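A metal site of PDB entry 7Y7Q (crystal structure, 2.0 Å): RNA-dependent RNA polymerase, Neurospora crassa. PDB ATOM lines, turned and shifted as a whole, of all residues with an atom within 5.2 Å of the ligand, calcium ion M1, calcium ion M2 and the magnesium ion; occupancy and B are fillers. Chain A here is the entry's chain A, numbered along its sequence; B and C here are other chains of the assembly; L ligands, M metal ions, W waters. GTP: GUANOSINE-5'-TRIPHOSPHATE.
The guanidinium group of Arg 586 sits at hydrogen-bond distance from an oxygen (O2') of the ligand (2.9 Å).
O2 of C 8 of chain B lies close to a nitrogen (N2) of the ligand (3.3 Å).
NZ of Lys 391 lies within salt-bridge range of O2G of the ligand.
The side-chain amino group (NZ) of Lys 743 lies within salt-bridge range of an oxygen (O1G) of the ligand, 3.0 Å away.
O2 of C 7 of chain B lies within hydrogen-bond range of N2 of the ligand (2.7 Å).
The guanidinium group (NH2) of Arg 295 lies within salt-bridge range of an oxygen (O2G) of the ligand (2.8 Å).
NZ of Lys 367 lies within salt-bridge range of OP1 of G 7 of chain C, 2.7 Å away.
The guanidinium group (NH1) of Arg 586 sits at hydrogen-bond distance from the backbone carbonyl oxygen (O) of Ser 628, at 3.0 Å.
OD2 of Asp 635 lies within salt-bridge range of NE of Arg 586.
The backbone carbonyl oxygen (O) of Pro 588 sits at hydrogen-bond distance from the side-chain hydroxyl (OG) of Ser 628, at 2.7 Å.
O2' of G 7 of chain C sits at hydrogen-bond distance from the guanidinium group (NH2) of Arg 586 (3.3 Å).
O6 of G 7 of chain C sits close to O6 of the ligand (3.3 Å).
Pro 588 touches the ligand.
Val 739 touches the ligand (CG2 to C4, 3.3 Å).
OD1 of Asp 740 touches C3' of the ligand, at 3.6 Å.
Hydrophobic or aromatic side chains that line the ligand: Pro 588 and Val 739.
The nearest printed residue that does not touch the ligand is Asp 635 (4.1 Å).
Within 4 Å of calcium ion M2: Asp 631 and Asp 633.
Gly 629 touches the magnesium ion.
Calcium ion M1 is bound by water W4 (2.3 Å).
Calcium ion M1 is bound by OD1 of Asp 631 (2.4 Å).
The side-chain carboxylate (OD1) of Asp 633 binds calcium ion M1.
Calcium ion M1 is bound by an oxygen (O2A) of the ligand.
Calcium ion M1 is bound by O2B of the ligand (2.7 Å).
OD1 of Asp 635 is bound to calcium ion M1, at 2.7 Å.
OD2 of Asp 633 binds calcium ion M1, at 2.8 Å.
OD2 of Asp 631 is bound to calcium ion M1 (2.8 Å).
Calcium ion M2 is bound by O3G of the ligand (2.1 Å).
Water W1 binds calcium ion M2, at 2.3 Å.
Calcium ion M2 is bound by O2B of the ligand, at 2.4 Å.
Water W5 is bound to calcium ion M2 (2.4 Å).
OD2 of Asp 631 is bound to calcium ion M2 (2.4 Å).
OD2 of Asp 633 binds calcium ion M2.
The magnesium ion is bound by the side-chain carboxylate (OD2) of Asp 631, at 2.5 Å.
The magnesium ion has one donor atom within binding distance.
Water W4 bridges the side-chain carboxylate (OD2) of Asp 635 (2.7 Å) and an oxygen (O5') of the ligand (3.4 Å).
Water W9 lies within hydrogen-bond range of O of Asp 633 (3.0 Å), OP1 of G 7 of chain C (3.1 Å) and NZ of Lys 367 (3.4 Å).
Water W8 lies within hydrogen-bond range of an oxygen (O2') of the ligand (2.8 Å) and the backbone carbonyl oxygen of Ser 628 (3.3 Å).
Water W3 bridges O6 of G 7 of chain C (2.7 Å) and O6 of the ligand (3.0 Å).
Water W7 lies within hydrogen-bond range of the side-chain amino group (NZ) of Lys 367 (2.5 Å), the side-chain amino group (NZ) of Lys 743 (2.9 Å) and an oxygen (O1G) of the ligand (3.0 Å).
Water W6 bridges OD1 of Asp 333 (2.7 Å) and NZ of Lys 391 (3.4 Å).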
ATOM      1  N   ARG A 295       8.593  16.428  32.712  1.00  0.00           N
ATOM      2  CA  ARG A 295       9.882  16.577  33.385  1.00  0.00           C
ATOM      3  C   ARG A 295      10.518  15.248  33.743  1.00  0.00           C
ATOM      4  O   ARG A 295      11.699  15.226  34.121  1.00  0.00           O
ATOM      5  CB  ARG A 295       9.728  17.445  34.635  1.00  0.00           C
ATOM      6  CG  ARG A 295       9.177  18.836  34.341  1.00  0.00           C
ATOM      7  CD  ARG A 295       9.920  19.468  33.179  1.00  0.00           C
ATOM      8  NE  ARG A 295       9.473  20.830  32.914  1.00  0.00           N
ATOM      9  CZ  ARG A 295       9.918  21.574  31.907  1.00  0.00           C
ATOM     10  NH1 ARG A 295      10.804  21.113  31.051  1.00  0.00           N
ATOM     11  NH2 ARG A 295       9.451  22.812  31.761  1.00  0.00           N
ATOM     12  N   ASP A 333      17.478  33.077  30.488  1.00  0.00           N
ATOM     13  CA  ASP A 333      16.612  31.870  30.580  1.00  0.00           C
ATOM     14  C   ASP A 333      17.402  30.614  30.213  1.00  0.00           C
ATOM     15  O   ASP A 333      17.763  30.477  29.050  1.00  0.00           O
ATOM     16  CB  ASP A 333      15.364  32.069  29.715  1.00  0.00           C
ATOM     17  CG  ASP A 333      14.329  30.961  29.803  1.00  0.00           C
ATOM     18  OD1 ASP A 333      14.513  30.041  30.592  1.00  0.00           O
ATOM     19  OD2 ASP A 333      13.344  31.047  29.053  1.00  0.00           O
ATOM     20  N   LYS A 367      18.055  22.340  34.396  1.00  0.00           N
ATOM     21  CA  LYS A 367      18.548  21.912  33.095  1.00  0.00           C
ATOM     22  C   LYS A 367      18.835  23.146  32.256  1.00  0.00           C
ATOM     23  O   LYS A 367      18.200  24.191  32.410  1.00  0.00           O
ATOM     24  CB  LYS A 367      17.543  21.000  32.373  1.00  0.00           C
ATOM     25  CG  LYS A 367      16.359  21.714  31.766  1.00  0.00           C
ATOM     26  CD  LYS A 367      16.351  21.536  30.252  1.00  0.00           C
ATOM     27  CE  LYS A 367      16.260  20.077  29.875  1.00  0.00           C
ATOM     28  NZ  LYS A 367      15.789  19.871  28.475  1.00  0.00           N
ATOM     29  N   LYS A 391      13.143  23.153  36.840  1.00  0.00           N
ATOM     30  CA  LYS A 391      11.855  22.735  36.307  1.00  0.00           C
ATOM     31  C   LYS A 391      10.919  22.165  37.367  1.00  0.00           C
ATOM     32  O   LYS A 391       9.754  21.875  37.051  1.00  0.00           O
ATOM     33  CB  LYS A 391      12.065  21.705  35.193  1.00  0.00           C
ATOM     34  CG  LYS A 391      12.927  22.216  34.047  1.00  0.00           C
ATOM     35  CD  LYS A 391      12.576  23.661  33.696  1.00  0.00           C
ATOM     36  CE  LYS A 391      13.323  24.123  32.454  1.00  0.00           C
ATOM     37  NZ  LYS A 391      12.936  25.501  32.060  1.00  0.00           N
ATOM     38  N   ARG A 586      17.299  30.384  14.620  1.00  0.00           N
ATOM     39  CA  ARG A 586      17.148  29.018  15.087  1.00  0.00           C
ATOM     40  C   ARG A 586      16.333  28.225  14.067  1.00  0.00           C
ATOM     41  O   ARG A 586      15.512  28.782  13.334  1.00  0.00           O
ATOM     42  CB  ARG A 586      16.457  28.952  16.451  1.00  0.00           C
ATOM     43  CG  ARG A 586      17.337  29.329  17.632  1.00  0.00           C
ATOM     44  CD  ARG A 586      16.585  29.158  18.955  1.00  0.00           C
ATOM     45  NE  ARG A 586      16.082  27.801  19.129  1.00  0.00           N
ATOM     46  CZ  ARG A 586      14.804  27.488  19.324  1.00  0.00           C
ATOM     47  NH1 ARG A 586      13.871  28.417  19.382  1.00  0.00           N
ATOM     48  NH2 ARG A 586      14.475  26.207  19.471  1.00  0.00           N
ATOM     49  N   SER A 587      16.571  26.923  14.038  1.00  0.00           N
ATOM     50  CA  SER A 587      15.662  26.045  13.316  1.00  0.00           C
ATOM     51  C   SER A 587      14.676  25.446  14.304  1.00  0.00           C
ATOM     52  O   SER A 587      15.083  24.993  15.376  1.00  0.00           O
ATOM     53  CB  SER A 587      16.440  24.924  12.622  1.00  0.00           C
ATOM     54  OG  SER A 587      17.659  25.406  12.088  1.00  0.00           O
ATOM     55  N   PRO A 588      13.366  25.421  13.980  1.00  0.00           N
ATOM     56  CA  PRO A 588      12.791  25.888  12.720  1.00  0.00           C
ATOM     57  C   PRO A 588      12.523  27.386  12.701  1.00  0.00           C
ATOM     58  O   PRO A 588      12.123  27.961  13.720  1.00  0.00           O
ATOM     59  CB  PRO A 588      11.480  25.116  12.648  1.00  0.00           C
ATOM     60  CG  PRO A 588      11.053  25.014  14.082  1.00  0.00           C
ATOM     61  CD  PRO A 588      12.335  24.890  14.886  1.00  0.00           C
ATOM     62  N   SER A 628      12.580  32.337  17.103  1.00  0.00           N
ATOM     63  CA  SER A 628      11.600  31.255  17.210  1.00  0.00           C
ATOM     64  C   SER A 628      11.349  30.878  18.672  1.00  0.00           C
ATOM     65  O   SER A 628      11.238  29.705  19.016  1.00  0.00           O
ATOM     66  CB  SER A 628      12.059  30.025  16.412  1.00  0.00           C
ATOM     67  OG  SER A 628      12.029  30.280  15.025  1.00  0.00           O
ATOM     68  N   GLY A 629      11.267  31.894  19.526  1.00  0.00           N
ATOM     69  CA  GLY A 629      11.025  31.665  20.946  1.00  0.00           C
ATOM     70  C   GLY A 629      12.161  30.988  21.672  1.00  0.00           C
ATOM     71  O   GLY A 629      11.918  30.231  22.618  1.00  0.00           O
ATOM     72  N   GLY A 630      13.404  31.257  21.270  1.00  0.00           N
ATOM     73  CA  GLY A 630      14.546  30.574  21.834  1.00  0.00           C
ATOM     74  C   GLY A 630      14.962  31.070  23.207  1.00  0.00           C
ATOM     75  O   GLY A 630      14.409  32.020  23.759  1.00  0.00           O
ATOM     76  N   ASP A 631      15.959  30.399  23.765  1.00  0.00           N
ATOM     77  CA  ASP A 631      16.497  30.746  25.069  1.00  0.00           C
ATOM     78  C   ASP A 631      17.933  30.219  25.126  1.00  0.00           C
ATOM     79  O   ASP A 631      18.540  29.939  24.088  1.00  0.00           O
ATOM     80  CB  ASP A 631      15.617  30.174  26.183  1.00  0.00           C
ATOM     81  CG  ASP A 631      15.298  28.706  25.994  1.00  0.00           C
ATOM     82  OD1 ASP A 631      16.194  27.960  25.551  1.00  0.00           O
ATOM     83  OD2 ASP A 631      14.149  28.303  26.272  1.00  0.00           O
ATOM     84  N   ASP A 633      19.167  27.460  27.028  1.00  0.00           N
ATOM     85  CA  ASP A 633      19.148  26.198  27.758  1.00  0.00           C
ATOM     86  C   ASP A 633      19.643  25.026  26.907  1.00  0.00           C
ATOM     87  O   ASP A 633      19.330  23.870  27.200  1.00  0.00           O
ATOM     88  CB  ASP A 633      17.732  25.923  28.290  1.00  0.00           C
ATOM     89  CG  ASP A 633      16.739  25.575  27.177  1.00  0.00           C
ATOM     90  OD1 ASP A 633      17.150  25.452  26.005  1.00  0.00           O
ATOM     91  OD2 ASP A 633      15.534  25.434  27.485  1.00  0.00           O
ATOM     92  N   ASP A 635      19.645  25.687  23.269  1.00  0.00           N
ATOM     93  CA  ASP A 635      19.371  26.162  21.921  1.00  0.00           C
ATOM     94  C   ASP A 635      20.684  26.485  21.208  1.00  0.00           C
ATOM     95  O   ASP A 635      21.650  26.955  21.821  1.00  0.00           O
ATOM     96  CB  ASP A 635      18.481  27.404  21.947  1.00  0.00           C
ATOM     97  CG  ASP A 635      17.059  27.100  22.370  1.00  0.00           C
ATOM     98  OD1 ASP A 635      16.801  25.957  22.820  1.00  0.00           O
ATOM     99  OD2 ASP A 635      16.204  28.007  22.284  1.00  0.00           O
ATOM    100  N   LEU A 706       1.802  18.205  14.098  1.00  0.00           N
ATOM    101  CA  LEU A 706       2.918  19.085  13.759  1.00  0.00           C
ATOM    102  C   LEU A 706       3.356  18.881  12.307  1.00  0.00           C
ATOM    103  O   LEU A 706       3.556  19.852  11.569  1.00  0.00           O
ATOM    104  CB  LEU A 706       4.085  18.838  14.709  1.00  0.00           C
ATOM    105  CG  LEU A 706       5.358  19.622  14.383  1.00  0.00           C
ATOM    106  CD1 LEU A 706       5.083  21.121  14.440  1.00  0.00           C
ATOM    107  CD2 LEU A 706       6.497  19.243  15.321  1.00  0.00           C
ATOM    108  N   VAL A 739       4.685  22.302  18.528  1.00  0.00           N
ATOM    109  CA  VAL A 739       5.962  21.702  18.901  1.00  0.00           C
ATOM    110  C   VAL A 739       6.063  21.560  20.416  1.00  0.00           C
ATOM    111  O   VAL A 739       6.608  20.578  20.926  1.00  0.00           O
ATOM    112  CB  VAL A 739       7.134  22.496  18.311  1.00  0.00           C
ATOM    113  CG1 VAL A 739       7.215  23.882  18.939  1.00  0.00           C
ATOM    114  CG2 VAL A 739       8.437  21.730  18.484  1.00  0.00           C
ATOM    115  N   ASP A 740       5.539  22.545  21.156  1.00  0.00           N
ATOM    116  CA  ASP A 740       5.552  22.535  22.621  1.00  0.00           C
ATOM    117  C   ASP A 740       4.335  21.824  23.212  1.00  0.00           C
ATOM    118  O   ASP A 740       3.950  22.121  24.344  1.00  0.00           O
ATOM    119  CB  ASP A 740       5.624  23.963  23.153  1.00  0.00           C
ATOM    120  CG  ASP A 740       6.675  24.813  22.452  1.00  0.00           C
ATOM    121  OD1 ASP A 740       7.858  24.422  22.463  1.00  0.00           O
ATOM    122  OD2 ASP A 740       6.308  25.859  21.887  1.00  0.00           O
ATOM    123  N   LYS A 743       4.575  19.592  26.599  1.00  0.00           N
ATOM    124  CA  LYS A 743       4.968  20.410  27.738  1.00  0.00           C
ATOM    125  C   LYS A 743       3.884  21.417  28.101  1.00  0.00           C
ATOM    126  O   LYS A 743       3.660  21.694  29.291  1.00  0.00           O
ATOM    127  CB  LYS A 743       6.280  21.126  27.448  1.00  0.00           C
ATOM    128  CG  LYS A 743       7.265  21.127  28.602  1.00  0.00           C
ATOM    129  CD  LYS A 743       8.651  21.545  28.146  1.00  0.00           C
ATOM    130  CE  LYS A 743       9.382  20.379  27.486  1.00  0.00           C
ATOM    131  NZ  LYS A 743      10.716  20.785  26.949  1.00  0.00           N
ATOM    132  P     C B   7       6.485  14.345   8.495  1.00  0.00           P
ATOM    133  OP1   C B   7       6.680  13.994   7.079  1.00  0.00           O
ATOM    134  OP2   C B   7       7.018  13.452   9.539  1.00  0.00           O
ATOM    135  O5'   C B   7       7.100  15.789   8.721  1.00  0.00           O
ATOM    136  C5'   C B   7       6.707  16.889   7.896  1.00  0.00           C
ATOM    137  C4'   C B   7       7.464  18.120   8.294  1.00  0.00           C
ATOM    138  O4'   C B   7       7.035  18.516   9.630  1.00  0.00           O
ATOM    139  C3'   C B   7       8.966  17.942   8.440  1.00  0.00           C
ATOM    140  O3'   C B   7       9.672  18.030   7.213  1.00  0.00           O
ATOM    141  C2'   C B   7       9.313  19.086   9.385  1.00  0.00           C
ATOM    142  O2'   C B   7       9.366  20.337   8.743  1.00  0.00           O
ATOM    143  C1'   C B   7       8.134  19.050  10.347  1.00  0.00           C
ATOM    144  N1    C B   7       8.358  18.227  11.530  1.00  0.00           N
ATOM    145  C2    C B   7       9.100  18.762  12.586  1.00  0.00           C
ATOM    146  O2    C B   7       9.539  19.920  12.479  1.00  0.00           O
ATOM    147  N3    C B   7       9.329  18.015  13.693  1.00  0.00           N
ATOM    148  C4    C B   7       8.835  16.781  13.769  1.00  0.00           C
ATOM    149  N4    C B   7       9.077  16.077  14.870  1.00  0.00           N
ATOM    150  C5    C B   7       8.080  16.198  12.710  1.00  0.00           C
ATOM    151  C6    C B   7       7.858  16.955  11.623  1.00  0.00           C
ATOM    152  P     C B   8      11.124  17.390   7.067  1.00  0.00           P
ATOM    153  OP1   C B   8      11.457  17.317   5.640  1.00  0.00           O
ATOM    154  OP2   C B   8      11.173  16.160   7.894  1.00  0.00           O
ATOM    155  O5'   C B   8      12.074  18.463   7.766  1.00  0.00           O
ATOM    156  C5'   C B   8      12.310  19.717   7.130  1.00  0.00           C
ATOM    157  C4'   C B   8      12.870  20.718   8.117  1.00  0.00           C
ATOM    158  O4'   C B   8      12.090  20.709   9.342  1.00  0.00           O
ATOM    159  C3'   C B   8      14.272  20.466   8.610  1.00  0.00           C
ATOM    160  O3'   C B   8      15.263  20.829   7.661  1.00  0.00           O
ATOM    161  C2'   C B   8      14.311  21.335   9.858  1.00  0.00           C
ATOM    162  O2'   C B   8      14.464  22.709   9.576  1.00  0.00           O
ATOM    163  C1'   C B   8      12.917  21.089  10.424  1.00  0.00           C
ATOM    164  N1    C B   8      12.881  20.024  11.440  1.00  0.00           N
ATOM    165  C2    C B   8      13.352  20.297  12.722  1.00  0.00           C
ATOM    166  O2    C B   8      13.771  21.439  12.972  1.00  0.00           O
ATOM    167  N3    C B   8      13.326  19.331  13.663  1.00  0.00           N
ATOM    168  C4    C B   8      12.862  18.124  13.357  1.00  0.00           C
ATOM    169  N4    C B   8      12.848  17.200  14.314  1.00  0.00           N
ATOM    170  C5    C B   8      12.380  17.804  12.050  1.00  0.00           C
ATOM    171  C6    C B   8      12.412  18.784  11.137  1.00  0.00           C
ATOM    172  P     G C   7      17.060  18.793  24.903  1.00  0.00           P
ATOM    173  OP1   G C   7      17.206  19.556  26.182  1.00  0.00           O
ATOM    174  OP2   G C   7      15.815  17.956  24.793  1.00  0.00           O
ATOM    175  O5'   G C   7      17.105  19.809  23.656  1.00  0.00           O
ATOM    176  C5'   G C   7      17.987  20.959  23.724  1.00  0.00           C
ATOM    177  C4'   G C   7      17.681  21.889  22.579  1.00  0.00           C
ATOM    178  O4'   G C   7      17.840  21.177  21.328  1.00  0.00           O
ATOM    179  C3'   G C   7      16.261  22.446  22.512  1.00  0.00           C
ATOM    180  C2'   G C   7      16.140  22.810  21.028  1.00  0.00           C
ATOM    181  O2'   G C   7      16.699  24.071  20.751  1.00  0.00           O
ATOM    182  C1'   G C   7      16.954  21.704  20.355  1.00  0.00           C
ATOM    183  N9    G C   7      16.167  20.609  19.804  1.00  0.00           N
ATOM    184  C8    G C   7      15.848  19.432  20.437  1.00  0.00           C
ATOM    185  N7    G C   7      15.154  18.617  19.699  1.00  0.00           N
ATOM    186  C5    G C   7      15.007  19.295  18.493  1.00  0.00           C
ATOM    187  C6    G C   7      14.345  18.896  17.301  1.00  0.00           C
ATOM    188  O6    G C   7      13.735  17.843  17.081  1.00  0.00           O
ATOM    189  N1    G C   7      14.433  19.874  16.322  1.00  0.00           N
ATOM    190  C2    G C   7      15.074  21.085  16.467  1.00  0.00           C
ATOM    191  N2    G C   7      15.065  21.899  15.399  1.00  0.00           N
ATOM    192  N3    G C   7      15.707  21.454  17.578  1.00  0.00           N
ATOM    193  C4    G C   7      15.623  20.518  18.551  1.00  0.00           C
HETATM  194  PG  GTP L   1      11.526  24.311  28.875  1.00  0.00           P
HETATM  195  O1G GTP L   1      11.827  22.854  28.782  1.00  0.00           O
HETATM  196  O2G GTP L   1      10.480  24.619  29.873  1.00  0.00           O
HETATM  197  O3G GTP L   1      12.757  25.135  29.055  1.00  0.00           O
HETATM  198  O3B GTP L   1      10.902  24.725  27.464  1.00  0.00           O
HETATM  199  PB  GTP L   1      11.540  24.962  26.027  1.00  0.00           P
HETATM  200  O1B GTP L   1      10.448  25.200  25.060  1.00  0.00           O
HETATM  201  O2B GTP L   1      12.641  25.943  26.127  1.00  0.00           O
HETATM  202  O3A GTP L   1      12.180  23.532  25.734  1.00  0.00           O
HETATM  203  PA  GTP L   1      13.300  23.043  24.706  1.00  0.00           P
HETATM  204  O1A GTP L   1      13.087  21.611  24.397  1.00  0.00           O
HETATM  205  O2A GTP L   1      14.629  23.478  25.195  1.00  0.00           O
HETATM  206  O5' GTP L   1      12.903  23.913  23.430  1.00  0.00           O
HETATM  207  C5' GTP L   1      11.812  23.452  22.605  1.00  0.00           C
HETATM  208  C4' GTP L   1      12.018  24.000  21.215  1.00  0.00           C
HETATM  209  O4' GTP L   1      12.912  23.113  20.491  1.00  0.00           O
HETATM  210  C3' GTP L   1      10.767  24.104  20.336  1.00  0.00           C
HETATM  211  C2' GTP L   1      11.384  24.023  18.936  1.00  0.00           C
HETATM  212  O2' GTP L   1      11.892  25.254  18.487  1.00  0.00           O
HETATM  213  C1' GTP L   1      12.493  22.987  19.153  1.00  0.00           C
HETATM  214  N9  GTP L   1      12.058  21.614  18.936  1.00  0.00           N
HETATM  215  C8  GTP L   1      12.011  20.604  19.860  1.00  0.00           C
HETATM  216  N7  GTP L   1      11.559  19.482  19.375  1.00  0.00           N
HETATM  217  C5  GTP L   1      11.285  19.766  18.045  1.00  0.00           C
HETATM  218  C6  GTP L   1      10.783  18.930  17.017  1.00  0.00           C
HETATM  219  O6  GTP L   1      10.455  17.738  17.091  1.00  0.00           O
HETATM  220  N1  GTP L   1      10.664  19.622  15.809  1.00  0.00           N
HETATM  221  C2  GTP L   1      10.991  20.941  15.624  1.00  0.00           C
HETATM  222  N2  GTP L   1      10.805  21.436  14.392  1.00  0.00           N
HETATM  223  N3  GTP L   1      11.467  21.729  16.580  1.00  0.00           N
HETATM  224  C4  GTP L   1      11.592  21.071  17.763  1.00  0.00           C
HETATM  225 CA    CA M   1      14.977  26.010  24.799  1.00  0.00          CA
HETATM  226 CA    CA M   2      13.610  26.861  28.145  1.00  0.00          CA
HETATM  227 MG    MG M   3      12.001  28.676  25.018  1.00  0.00          MG
HETATM  228  O   HOH W   1      12.019  28.578  28.191  1.00  0.00           O
HETATM  229  O   HOH W   2      11.941  31.758  24.987  1.00  0.00           O
HETATM  230  O   HOH W   3      12.410  15.894  18.332  1.00  0.00           O
HETATM  231  O   HOH W   4      13.822  27.222  23.292  1.00  0.00           O
HETATM  232  O   HOH W   5      15.042  27.550  29.975  1.00  0.00           O
HETATM  233  O   HOH W   6      12.271  28.557  30.649  1.00  0.00           O
HETATM  234  O   HOH W   7      13.569  20.690  27.654  1.00  0.00           O
HETATM  235  O   HOH W   8       9.822  26.996  17.803  1.00  0.00           O
HETATM  236  O   HOH W   9      16.753  22.551  26.600  1.00  0.00           O
HETATM  237  O   HOH W  10      10.412  26.818  23.026  1.00  0.00           O
